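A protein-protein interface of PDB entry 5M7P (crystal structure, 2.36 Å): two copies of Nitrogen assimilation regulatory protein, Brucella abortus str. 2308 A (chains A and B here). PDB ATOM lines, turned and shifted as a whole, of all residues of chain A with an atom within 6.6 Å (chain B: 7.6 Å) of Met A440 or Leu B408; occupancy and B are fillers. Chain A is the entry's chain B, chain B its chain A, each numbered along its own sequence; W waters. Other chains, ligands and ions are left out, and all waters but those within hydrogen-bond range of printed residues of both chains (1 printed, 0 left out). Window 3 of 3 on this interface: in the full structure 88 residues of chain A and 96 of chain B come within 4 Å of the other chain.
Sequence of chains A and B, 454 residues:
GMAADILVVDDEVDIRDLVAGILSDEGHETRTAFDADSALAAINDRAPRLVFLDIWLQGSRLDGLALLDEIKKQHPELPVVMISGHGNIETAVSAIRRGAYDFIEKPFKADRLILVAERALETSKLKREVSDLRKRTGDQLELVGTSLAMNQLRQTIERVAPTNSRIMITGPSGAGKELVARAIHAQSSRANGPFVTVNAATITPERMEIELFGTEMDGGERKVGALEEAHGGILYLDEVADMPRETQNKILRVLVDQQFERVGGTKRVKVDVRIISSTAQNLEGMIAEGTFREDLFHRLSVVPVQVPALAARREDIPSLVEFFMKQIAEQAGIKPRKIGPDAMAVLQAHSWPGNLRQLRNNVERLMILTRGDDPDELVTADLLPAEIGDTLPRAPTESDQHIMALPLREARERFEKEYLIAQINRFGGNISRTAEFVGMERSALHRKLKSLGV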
ATOM      1  N   PHE A 415      29.885 -19.806   2.667  1.00  0.00           N
ATOM      2  CA  PHE A 415      28.836 -20.726   3.126  1.00  0.00           C
ATOM      3  C   PHE A 415      27.710 -19.956   3.813  1.00  0.00           C
ATOM      4  O   PHE A 415      26.543 -20.227   3.539  1.00  0.00           O
ATOM      5  CB  PHE A 415      29.394 -21.818   4.072  1.00  0.00           C
ATOM      6  CG  PHE A 415      28.297 -22.663   4.694  1.00  0.00           C
ATOM      7  CD1 PHE A 415      27.669 -22.262   5.873  1.00  0.00           C
ATOM      8  CD2 PHE A 415      27.858 -23.832   4.074  1.00  0.00           C
ATOM      9  CE1 PHE A 415      26.612 -22.999   6.407  1.00  0.00           C
ATOM     10  CE2 PHE A 415      26.832 -24.595   4.639  1.00  0.00           C
ATOM     11  CZ  PHE A 415      26.214 -24.170   5.801  1.00  0.00           C
ATOM     12  N   GLU A 416      28.068 -19.017   4.720  1.00  0.00           N
ATOM     13  CA  GLU A 416      27.111 -18.210   5.487  1.00  0.00           C
ATOM     14  C   GLU A 416      26.199 -17.378   4.570  1.00  0.00           C
ATOM     15  O   GLU A 416      24.988 -17.360   4.751  1.00  0.00           O
ATOM     16  CB  GLU A 416      27.848 -17.304   6.482  1.00  0.00           C
ATOM     17  CG  GLU A 416      28.288 -18.003   7.750  1.00  0.00           C
ATOM     18  CD  GLU A 416      28.704 -17.029   8.832  1.00  0.00           C
ATOM     19  OE1 GLU A 416      29.773 -16.392   8.693  1.00  0.00           O
ATOM     20  OE2 GLU A 416      27.948 -16.894   9.820  1.00  0.00           O
ATOM     21  N   TYR A 419      23.952 -19.816   2.444  1.00  0.00           N
ATOM     22  CA  TYR A 419      22.979 -20.401   3.358  1.00  0.00           C
ATOM     23  C   TYR A 419      21.841 -19.387   3.608  1.00  0.00           C
ATOM     24  O   TYR A 419      20.671 -19.770   3.603  1.00  0.00           O
ATOM     25  CB  TYR A 419      23.678 -20.754   4.694  1.00  0.00           C
ATOM     26  CG  TYR A 419      22.719 -21.047   5.827  1.00  0.00           C
ATOM     27  CD1 TYR A 419      22.210 -22.327   6.020  1.00  0.00           C
ATOM     28  CD2 TYR A 419      22.291 -20.036   6.683  1.00  0.00           C
ATOM     29  CE1 TYR A 419      21.315 -22.600   7.048  1.00  0.00           C
ATOM     30  CE2 TYR A 419      21.389 -20.296   7.710  1.00  0.00           C
ATOM     31  CZ  TYR A 419      20.922 -21.584   7.902  1.00  0.00           C
ATOM     32  OH  TYR A 419      20.044 -21.849   8.912  1.00  0.00           O
ATOM     33  N   LEU A 420      22.189 -18.116   3.894  1.00  0.00           N
ATOM     34  CA  LEU A 420      21.184 -17.095   4.179  1.00  0.00           C
ATOM     35  C   LEU A 420      20.371 -16.764   2.937  1.00  0.00           C
ATOM     36  O   LEU A 420      19.154 -16.675   3.041  1.00  0.00           O
ATOM     37  CB  LEU A 420      21.778 -15.834   4.846  1.00  0.00           C
ATOM     38  CG  LEU A 420      22.412 -16.012   6.242  1.00  0.00           C
ATOM     39  CD1 LEU A 420      23.251 -14.810   6.617  1.00  0.00           C
ATOM     40  CD2 LEU A 420      21.388 -16.329   7.321  1.00  0.00           C
ATOM     41  N   GLN A 423      17.970 -19.570   2.450  1.00  0.00           N
ATOM     42  CA  GLN A 423      16.916 -19.560   3.476  1.00  0.00           C
ATOM     43  C   GLN A 423      15.878 -18.467   3.191  1.00  0.00           C
ATOM     44  O   GLN A 423      14.702 -18.667   3.479  1.00  0.00           O
ATOM     45  CB  GLN A 423      17.484 -19.431   4.907  1.00  0.00           C
ATOM     46  CG  GLN A 423      18.199 -20.679   5.443  1.00  0.00           C
ATOM     47  CD  GLN A 423      17.312 -21.797   5.962  1.00  0.00           C
ATOM     48  OE1 GLN A 423      16.095 -21.828   5.758  1.00  0.00           O
ATOM     49  NE2 GLN A 423      17.915 -22.759   6.654  1.00  0.00           N
ATOM     50  N   SER A 432      11.833 -11.446   8.413  1.00  0.00           N
ATOM     51  CA  SER A 432      11.470 -11.694   9.819  1.00  0.00           C
ATOM     52  C   SER A 432      11.291 -13.183  10.174  1.00  0.00           C
ATOM     53  O   SER A 432      11.645 -13.591  11.286  1.00  0.00           O
ATOM     54  CB  SER A 432      10.235 -10.891  10.221  1.00  0.00           C
ATOM     55  OG  SER A 432       9.034 -11.456   9.721  1.00  0.00           O
ATOM     56  N   THR A 434      12.663 -15.647   8.296  1.00  0.00           N
ATOM     57  CA  THR A 434      13.964 -16.235   7.978  1.00  0.00           C
ATOM     58  C   THR A 434      14.846 -16.063   9.214  1.00  0.00           C
ATOM     59  O   THR A 434      15.412 -17.044   9.691  1.00  0.00           O
ATOM     60  CB  THR A 434      14.594 -15.595   6.723  1.00  0.00           C
ATOM     61  OG1 THR A 434      13.671 -15.662   5.637  1.00  0.00           O
ATOM     62  CG2 THR A 434      15.909 -16.264   6.326  1.00  0.00           C
ATOM     63  N   ALA A 435      14.892 -14.826   9.751  1.00  0.00           N
ATOM     64  CA  ALA A 435      15.630 -14.432  10.936  1.00  0.00           C
ATOM     65  C   ALA A 435      15.299 -15.367  12.089  1.00  0.00           C
ATOM     66  O   ALA A 435      16.205 -15.991  12.636  1.00  0.00           O
ATOM     67  CB  ALA A 435      15.308 -12.982  11.298  1.00  0.00           C
ATOM     68  N   GLU A 436      13.997 -15.535  12.384  1.00  0.00           N
ATOM     69  CA  GLU A 436      13.479 -16.391  13.447  1.00  0.00           C
ATOM     70  C   GLU A 436      13.926 -17.840  13.284  1.00  0.00           C
ATOM     71  O   GLU A 436      14.339 -18.457  14.270  1.00  0.00           O
ATOM     72  CB  GLU A 436      11.945 -16.280  13.544  1.00  0.00           C
ATOM     73  CG  GLU A 436      11.374 -16.883  14.824  1.00  0.00           C
ATOM     74  CD  GLU A 436      10.056 -16.339  15.349  1.00  0.00           C
ATOM     75  OE1 GLU A 436       9.509 -15.380  14.755  1.00  0.00           O
ATOM     76  OE2 GLU A 436       9.581 -16.868  16.379  1.00  0.00           O
ATOM     77  N   PHE A 437      13.844 -18.377  12.047  1.00  0.00           N
ATOM     78  CA  PHE A 437      14.251 -19.749  11.742  1.00  0.00           C
ATOM     79  C   PHE A 437      15.780 -19.952  11.825  1.00  0.00           C
ATOM     80  O   PHE A 437      16.221 -20.991  12.327  1.00  0.00           O
ATOM     81  CB  PHE A 437      13.719 -20.219  10.373  1.00  0.00           C
ATOM     82  CG  PHE A 437      14.133 -21.643  10.085  1.00  0.00           C
ATOM     83  CD1 PHE A 437      13.361 -22.709  10.532  1.00  0.00           C
ATOM     84  CD2 PHE A 437      15.357 -21.922   9.480  1.00  0.00           C
ATOM     85  CE1 PHE A 437      13.789 -24.025  10.350  1.00  0.00           C
ATOM     86  CE2 PHE A 437      15.802 -23.235   9.336  1.00  0.00           C
ATOM     87  CZ  PHE A 437      15.004 -24.279   9.742  1.00  0.00           C
ATOM     88  N   VAL A 438      16.581 -18.989  11.320  1.00  0.00           N
ATOM     89  CA  VAL A 438      18.043 -19.120  11.316  1.00  0.00           C
ATOM     90  C   VAL A 438      18.651 -18.875  12.704  1.00  0.00           C
ATOM     91  O   VAL A 438      19.793 -19.264  12.936  1.00  0.00           O
ATOM     92  CB  VAL A 438      18.766 -18.319  10.199  1.00  0.00           C
ATOM     93  CG1 VAL A 438      18.257 -18.733   8.818  1.00  0.00           C
ATOM     94  CG2 VAL A 438      18.667 -16.815  10.398  1.00  0.00           C
ATOM     95  N   GLY A 439      17.879 -18.271  13.606  1.00  0.00           N
ATOM     96  CA  GLY A 439      18.294 -17.994  14.974  1.00  0.00           C
ATOM     97  C   GLY A 439      18.826 -16.598  15.181  1.00  0.00           C
ATOM     98  O   GLY A 439      19.608 -16.355  16.102  1.00  0.00           O
ATOM     99  N   MET A 440      18.399 -15.672  14.326  1.00  0.00           N
ATOM    100  CA  MET A 440      18.812 -14.280  14.376  1.00  0.00           C
ATOM    101  C   MET A 440      17.639 -13.322  14.685  1.00  0.00           C
ATOM    102  O   MET A 440      16.467 -13.651  14.458  1.00  0.00           O
ATOM    103  CB  MET A 440      19.464 -13.870  13.034  1.00  0.00           C
ATOM    104  CG  MET A 440      20.806 -14.539  12.757  1.00  0.00           C
ATOM    105  SD  MET A 440      21.684 -13.802  11.344  1.00  0.00           S
ATOM    106  CE  MET A 440      22.455 -12.405  12.119  1.00  0.00           C
ATOM    107  N   GLU A 441      17.985 -12.119  15.183  1.00  0.00           N
ATOM    108  CA  GLU A 441      17.074 -10.996  15.391  1.00  0.00           C
ATOM    109  C   GLU A 441      17.019 -10.265  14.012  1.00  0.00           C
ATOM    110  O   GLU A 441      18.039 -10.205  13.316  1.00  0.00           O
ATOM    111  CB  GLU A 441      17.606 -10.090  16.521  1.00  0.00           C
ATOM    112  CG  GLU A 441      16.785  -8.847  16.812  1.00  0.00           C
ATOM    113  CD  GLU A 441      17.106  -7.667  15.911  1.00  0.00           C
ATOM    114  OE1 GLU A 441      18.302  -7.463  15.597  1.00  0.00           O
ATOM    115  OE2 GLU A 441      16.161  -6.962  15.496  1.00  0.00           O
ATOM    116  N   ARG A 442      15.827  -9.728  13.625  1.00  0.00           N
ATOM    117  CA  ARG A 442      15.547  -9.075  12.329  1.00  0.00           C
ATOM    118  C   ARG A 442      16.631  -8.114  11.841  1.00  0.00           C
ATOM    119  O   ARG A 442      17.140  -8.313  10.741  1.00  0.00           O
ATOM    120  CB  ARG A 442      14.172  -8.365  12.317  1.00  0.00           C
ATOM    121  CG  ARG A 442      12.988  -9.296  12.624  1.00  0.00           C
ATOM    122  CD  ARG A 442      11.646  -8.583  12.769  1.00  0.00           C
ATOM    123  NE  ARG A 442      11.640  -7.592  13.849  1.00  0.00           N
ATOM    124  CZ  ARG A 442      11.312  -7.845  15.116  1.00  0.00           C
ATOM    125  NH1 ARG A 442      11.344  -6.874  16.021  1.00  0.00           N
ATOM    126  NH2 ARG A 442      10.948  -9.069  15.486  1.00  0.00           N
ATOM    127  N   SER A 443      16.967  -7.071  12.630  1.00  0.00           N
ATOM    128  CA  SER A 443      17.958  -6.064  12.236  1.00  0.00           C
ATOM    129  C   SER A 443      19.385  -6.634  12.095  1.00  0.00           C
ATOM    130  O   SER A 443      20.132  -6.187  11.224  1.00  0.00           O
ATOM    131  CB  SER A 443      17.917  -4.858  13.171  1.00  0.00           C
ATOM    132  OG  SER A 443      18.550  -5.107  14.417  1.00  0.00           O
ATOM    133  N   ALA A 444      19.742  -7.629  12.942  1.00  0.00           N
ATOM    134  CA  ALA A 444      21.023  -8.325  12.905  1.00  0.00           C
ATOM    135  C   ALA A 444      21.181  -9.068  11.560  1.00  0.00           C
ATOM    136  O   ALA A 444      22.262  -9.020  10.973  1.00  0.00           O
ATOM    137  CB  ALA A 444      21.129  -9.291  14.077  1.00  0.00           C
ATOM    138  N   LEU A 445      20.095  -9.703  11.050  1.00  0.00           N
ATOM    139  CA  LEU A 445      20.113 -10.384   9.751  1.00  0.00           C
ATOM    140  C   LEU A 445      20.359  -9.372   8.630  1.00  0.00           C
ATOM    141  O   LEU A 445      21.219  -9.628   7.782  1.00  0.00           O
ATOM    142  CB  LEU A 445      18.838 -11.214   9.509  1.00  0.00           C
ATOM    143  CG  LEU A 445      18.693 -11.903   8.133  1.00  0.00           C
ATOM    144  CD1 LEU A 445      19.885 -12.798   7.806  1.00  0.00           C
ATOM    145  CD2 LEU A 445      17.410 -12.702   8.059  1.00  0.00           C
ATOM    146  N   HIS A 446      19.674  -8.197   8.687  1.00  0.00           N
ATOM    147  CA  HIS A 446      19.830  -7.081   7.753  1.00  0.00           C
ATOM    148  C   HIS A 446      21.272  -6.641   7.680  1.00  0.00           C
ATOM    149  O   HIS A 446      21.828  -6.625   6.583  1.00  0.00           O
ATOM    150  CB  HIS A 446      18.960  -5.877   8.155  1.00  0.00           C
ATOM    151  CG  HIS A 446      17.517  -6.010   7.783  1.00  0.00           C
ATOM    152  ND1 HIS A 446      17.108  -6.034   6.452  1.00  0.00           N
ATOM    153  CD2 HIS A 446      16.424  -6.079   8.576  1.00  0.00           C
ATOM    154  CE1 HIS A 446      15.788  -6.145   6.487  1.00  0.00           C
ATOM    155  NE2 HIS A 446      15.330  -6.180   7.741  1.00  0.00           N
ATOM    156  N   LYS A 448      23.951  -8.278   8.765  1.00  0.00           N
ATOM    157  CA  LYS A 448      24.805  -9.404   8.347  1.00  0.00           C
ATOM    158  C   LYS A 448      24.778  -9.543   6.822  1.00  0.00           C
ATOM    159  O   LYS A 448      25.848  -9.648   6.216  1.00  0.00           O
ATOM    160  CB  LYS A 448      24.410 -10.726   9.049  1.00  0.00           C
ATOM    161  CG  LYS A 448      25.285 -11.912   8.655  1.00  0.00           C
ATOM    162  CD  LYS A 448      25.339 -12.978   9.731  1.00  0.00           C
ATOM    163  CE  LYS A 448      26.240 -14.123   9.342  1.00  0.00           C
ATOM    164  NZ  LYS A 448      27.676 -13.742   9.365  1.00  0.00           N
ATOM    165  N   ILE B 403      20.921 -29.109   5.487  1.00  0.00           N
ATOM    166  CA  ILE B 403      21.446 -27.773   5.818  1.00  0.00           C
ATOM    167  C   ILE B 403      20.291 -26.830   6.147  1.00  0.00           C
ATOM    168  O   ILE B 403      20.362 -26.090   7.130  1.00  0.00           O
ATOM    169  CB  ILE B 403      22.330 -27.174   4.673  1.00  0.00           C
ATOM    170  CG1 ILE B 403      23.325 -28.207   4.076  1.00  0.00           C
ATOM    171  CG2 ILE B 403      23.039 -25.877   5.112  1.00  0.00           C
ATOM    172  CD1 ILE B 403      24.581 -28.513   4.874  1.00  0.00           C
ATOM    173  N   LEU B 406      18.573 -26.953   9.528  1.00  0.00           N
ATOM    174  CA  LEU B 406      19.426 -26.450  10.609  1.00  0.00           C
ATOM    175  C   LEU B 406      19.473 -24.917  10.714  1.00  0.00           C
ATOM    176  O   LEU B 406      19.580 -24.267   9.678  1.00  0.00           O
ATOM    177  CB  LEU B 406      20.874 -26.950  10.416  1.00  0.00           C
ATOM    178  CG  LEU B 406      21.145 -28.438  10.576  1.00  0.00           C
ATOM    179  CD1 LEU B 406      22.509 -28.777  10.053  1.00  0.00           C
ATOM    180  CD2 LEU B 406      20.999 -28.884  12.027  1.00  0.00           C
ATOM    181  N   PRO B 407      19.521 -24.331  11.944  1.00  0.00           N
ATOM    182  CA  PRO B 407      19.698 -22.867  12.062  1.00  0.00           C
ATOM    183  C   PRO B 407      21.153 -22.466  11.718  1.00  0.00           C
ATOM    184  O   PRO B 407      21.981 -23.343  11.495  1.00  0.00           O
ATOM    185  CB  PRO B 407      19.336 -22.569  13.534  1.00  0.00           C
ATOM    186  CG  PRO B 407      18.796 -23.868  14.102  1.00  0.00           C
ATOM    187  CD  PRO B 407      19.435 -24.957  13.278  1.00  0.00           C
ATOM    188  N   LEU B 408      21.466 -21.162  11.679  1.00  0.00           N
ATOM    189  CA  LEU B 408      22.772 -20.639  11.288  1.00  0.00           C
ATOM    190  C   LEU B 408      23.989 -21.235  12.027  1.00  0.00           C
ATOM    191  O   LEU B 408      24.887 -21.717  11.332  1.00  0.00           O
ATOM    192  CB  LEU B 408      22.806 -19.097  11.353  1.00  0.00           C
ATOM    193  CG  LEU B 408      24.131 -18.378  10.984  1.00  0.00           C
ATOM    194  CD1 LEU B 408      24.595 -18.706   9.549  1.00  0.00           C
ATOM    195  CD2 LEU B 408      23.972 -16.893  11.131  1.00  0.00           C
ATOM    196  N   ARG B 409      24.056 -21.173  13.385  1.00  0.00           N
ATOM    197  CA  ARG B 409      25.211 -21.691  14.145  1.00  0.00           C
ATOM    198  C   ARG B 409      25.447 -23.186  13.910  1.00  0.00           C
ATOM    199  O   ARG B 409      26.588 -23.591  13.723  1.00  0.00           O
ATOM    200  CB  ARG B 409      25.095 -21.395  15.664  1.00  0.00           C
ATOM    201  CG  ARG B 409      26.420 -21.631  16.430  1.00  0.00           C
ATOM    202  CD  ARG B 409      26.383 -21.312  17.925  1.00  0.00           C
ATOM    203  NE  ARG B 409      25.238 -21.944  18.581  1.00  0.00           N
ATOM    204  CZ  ARG B 409      25.234 -23.167  19.091  1.00  0.00           C
ATOM    205  NH1 ARG B 409      26.341 -23.902  19.090  1.00  0.00           N
ATOM    206  NH2 ARG B 409      24.122 -23.664  19.621  1.00  0.00           N
ATOM    207  N   GLU B 410      24.378 -23.996  13.926  1.00  0.00           N
ATOM    208  CA  GLU B 410      24.452 -25.441  13.721  1.00  0.00           C
ATOM    209  C   GLU B 410      24.916 -25.748  12.302  1.00  0.00           C
ATOM    210  O   GLU B 410      25.774 -26.618  12.126  1.00  0.00           O
ATOM    211  CB  GLU B 410      23.100 -26.122  14.020  1.00  0.00           C
ATOM    212  CG  GLU B 410      22.731 -26.139  15.495  1.00  0.00           C
ATOM    213  CD  GLU B 410      22.100 -24.889  16.086  1.00  0.00           C
ATOM    214  OE1 GLU B 410      21.925 -23.883  15.360  1.00  0.00           O
ATOM    215  OE2 GLU B 410      21.791 -24.918  17.297  1.00  0.00           O
ATOM    216  N   ALA B 411      24.398 -24.993  11.304  1.00  0.00           N
ATOM    217  CA  ALA B 411      24.743 -25.174   9.897  1.00  0.00           C
ATOM    218  C   ALA B 411      26.191 -24.790   9.619  1.00  0.00           C
ATOM    219  O   ALA B 411      26.872 -25.518   8.909  1.00  0.00           O
ATOM    220  CB  ALA B 411      23.791 -24.388   9.019  1.00  0.00           C
ATOM    221  N   ARG B 412      26.682 -23.693  10.239  1.00  0.00           N
ATOM    222  CA  ARG B 412      28.067 -23.195  10.150  1.00  0.00           C
ATOM    223  C   ARG B 412      29.049 -24.179  10.836  1.00  0.00           C
ATOM    224  O   ARG B 412      30.140 -24.429  10.306  1.00  0.00           O
ATOM    225  CB  ARG B 412      28.140 -21.811  10.798  1.00  0.00           C
ATOM    226  CG  ARG B 412      29.468 -21.079  10.653  1.00  0.00           C
ATOM    227  CD  ARG B 412      29.345 -19.659  11.173  1.00  0.00           C
ATOM    228  NE  ARG B 412      28.972 -19.630  12.586  1.00  0.00           N
ATOM    229  CZ  ARG B 412      28.166 -18.732  13.145  1.00  0.00           C
ATOM    230  NH1 ARG B 412      27.617 -17.771  12.408  1.00  0.00           N
ATOM    231  NH2 ARG B 412      27.894 -18.793  14.442  1.00  0.00           N
ATOM    232  N   GLU B 413      28.654 -24.761  11.982  1.00  0.00           N
ATOM    233  CA  GLU B 413      29.482 -25.762  12.673  1.00  0.00           C
ATOM    234  C   GLU B 413      29.617 -27.049  11.854  1.00  0.00           C
ATOM    235  O   GLU B 413      30.718 -27.586  11.752  1.00  0.00           O
ATOM    236  CB  GLU B 413      28.952 -26.068  14.077  1.00  0.00           C
ATOM    237  CG  GLU B 413      29.296 -24.961  15.062  1.00  0.00           C
ATOM    238  CD  GLU B 413      28.549 -24.951  16.383  1.00  0.00           C
ATOM    239  OE1 GLU B 413      27.822 -25.929  16.685  1.00  0.00           O
ATOM    240  OE2 GLU B 413      28.704 -23.953  17.124  1.00  0.00           O
ATOM    241  N   ARG B 414      28.501 -27.519  11.248  1.00  0.00           N
ATOM    242  CA  ARG B 414      28.475 -28.697  10.381  1.00  0.00           C
ATOM    243  C   ARG B 414      29.366 -28.437   9.159  1.00  0.00           C
ATOM    244  O   ARG B 414      30.137 -29.316   8.788  1.00  0.00           O
ATOM    245  CB  ARG B 414      27.037 -29.023   9.938  1.00  0.00           C
ATOM    246  CG  ARG B 414      26.853 -30.407   9.320  1.00  0.00           C
ATOM    247  CD  ARG B 414      25.487 -30.470   8.681  1.00  0.00           C
ATOM    248  NE  ARG B 414      25.134 -31.791   8.162  1.00  0.00           N
ATOM    249  CZ  ARG B 414      25.182 -32.134   6.877  1.00  0.00           C
ATOM    250  NH1 ARG B 414      25.623 -31.276   5.968  1.00  0.00           N
ATOM    251  NH2 ARG B 414      24.819 -33.352   6.496  1.00  0.00           N
ATOM    252  N   PHE B 415      29.293 -27.214   8.574  1.00  0.00           N
ATOM    253  CA  PHE B 415      30.128 -26.869   7.441  1.00  0.00           C
ATOM    254  C   PHE B 415      31.604 -26.891   7.868  1.00  0.00           C
ATOM    255  O   PHE B 415      32.432 -27.422   7.136  1.00  0.00           O
ATOM    256  CB  PHE B 415      29.745 -25.498   6.852  1.00  0.00           C
ATOM    257  CG  PHE B 415      30.831 -24.932   5.966  1.00  0.00           C
ATOM    258  CD1 PHE B 415      30.968 -25.360   4.650  1.00  0.00           C
ATOM    259  CD2 PHE B 415      31.768 -24.040   6.472  1.00  0.00           C
ATOM    260  CE1 PHE B 415      31.997 -24.879   3.850  1.00  0.00           C
ATOM    261  CE2 PHE B 415      32.816 -23.580   5.679  1.00  0.00           C
ATOM    262  CZ  PHE B 415      32.917 -23.991   4.368  1.00  0.00           C
HETATM  263  O   HOH W   1      21.769 -19.514  14.850  1.00  0.00           O
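Phe A415 touches Ile B403. CZ of Phe A415 touches O of Ala B411, at 3.5 Å. Phe A415 touches Arg B412. Phe A415 touches Phe B415. Tyr A419 touches Ile B403. OH of Tyr A419 touches C of Pro B407, at 3.1 Å. CB of Ala B411 touches CE1 of Tyr A419 (3.6 Å). Leu B406 touches Gln A423. CE2 of Phe A437 touches O of Leu B406, at 3.9 Å. Met A440 touches Leu B408 (SD to CD2, 3.9 Å).
Phe A415 touches its own counterpart, Phe B415.
Of the printed residues of chain B, Phe A437 touches Leu B406 and Pro B407. No residue of chain B comes within 4 Å of Gly A439. Of chain B, only Leu B408 comes within 4 Å of Met A440. Glu A441 touches none of the printed residues of chain B. Ser A443 touches none of the printed residues of chain B. Printed residues of chain A within 4 Å of Leu B406: Tyr A419 (2.6 Å), Gln A423 (3.8 Å) and Phe A437 (3.9 Å). Of the printed residues of chain A, Arg B412 touches Phe A415 (3.9 Å) and Glu A416 (2.8 Å). The nearest printed residue of chain A that does not touch Leu B408 is Lys A448 (4.002 Å).
Printed residues of chain A that touch a printed residue of chain B: Phe A415, Glu A416, Tyr A419, Gln A423, Phe A437, Val A438 and Met A440. Hydrophobic or aromatic side chains of chain A within 4 Å of the printed part of chain B: Phe A415, Tyr A419, Phe A437 and Met A440. Printed residues of chain B that touch a printed residue of chain A: Ile B403, Leu B406, Pro B407, Leu B408, Ala B411, Arg B412 and Phe B415. Hydrophobic or aromatic side chains of chain B that line the printed part of chain A: Ile B403, Pro B407, Leu B408, Ala B411 and Phe B415. Among the printed residues, 17 pairs touch across the chains. Among the printed residues, Asp or Glu carboxylates within 4 Å of a Lys or Arg side-chain nitrogen of the other chain: Glu A416 with Arg B412.
The backbone NH of Leu B408 is in hydrogen-bond range of the backbone carbonyl oxygen of Val A438 (2.8 Å). NH1 of Arg B412 lies within salt-bridge range of OE2 of Glu A416 (2.8 Å). The backbone carbonyl oxygen (O) of Leu B406 sits at hydrogen-bond distance from the side-chain hydroxyl (OH) of Tyr A419 (2.6 Å). OH of Tyr A419 sits at hydrogen-bond distance from N of Leu B408 (3.2 Å).
The backbone carbonyl oxygen of Ala A435 lies within hydrogen-bond range of the backbone NH of Met A440, at 2.8 Å. The side-chain amino group of Lys A448 lies within salt-bridge range of the side-chain carboxylate of Glu A416 (3.2 Å). The side-chain hydroxyl of Tyr A419 is in hydrogen-bond range of the side-chain amide nitrogen of Gln A423, 3.2 Å away.
Water W1 lies within hydrogen-bond range of the backbone carbonyl oxygen of Val A438 (2.8 Å) and the backbone NH of Arg B409 (3.2 Å).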
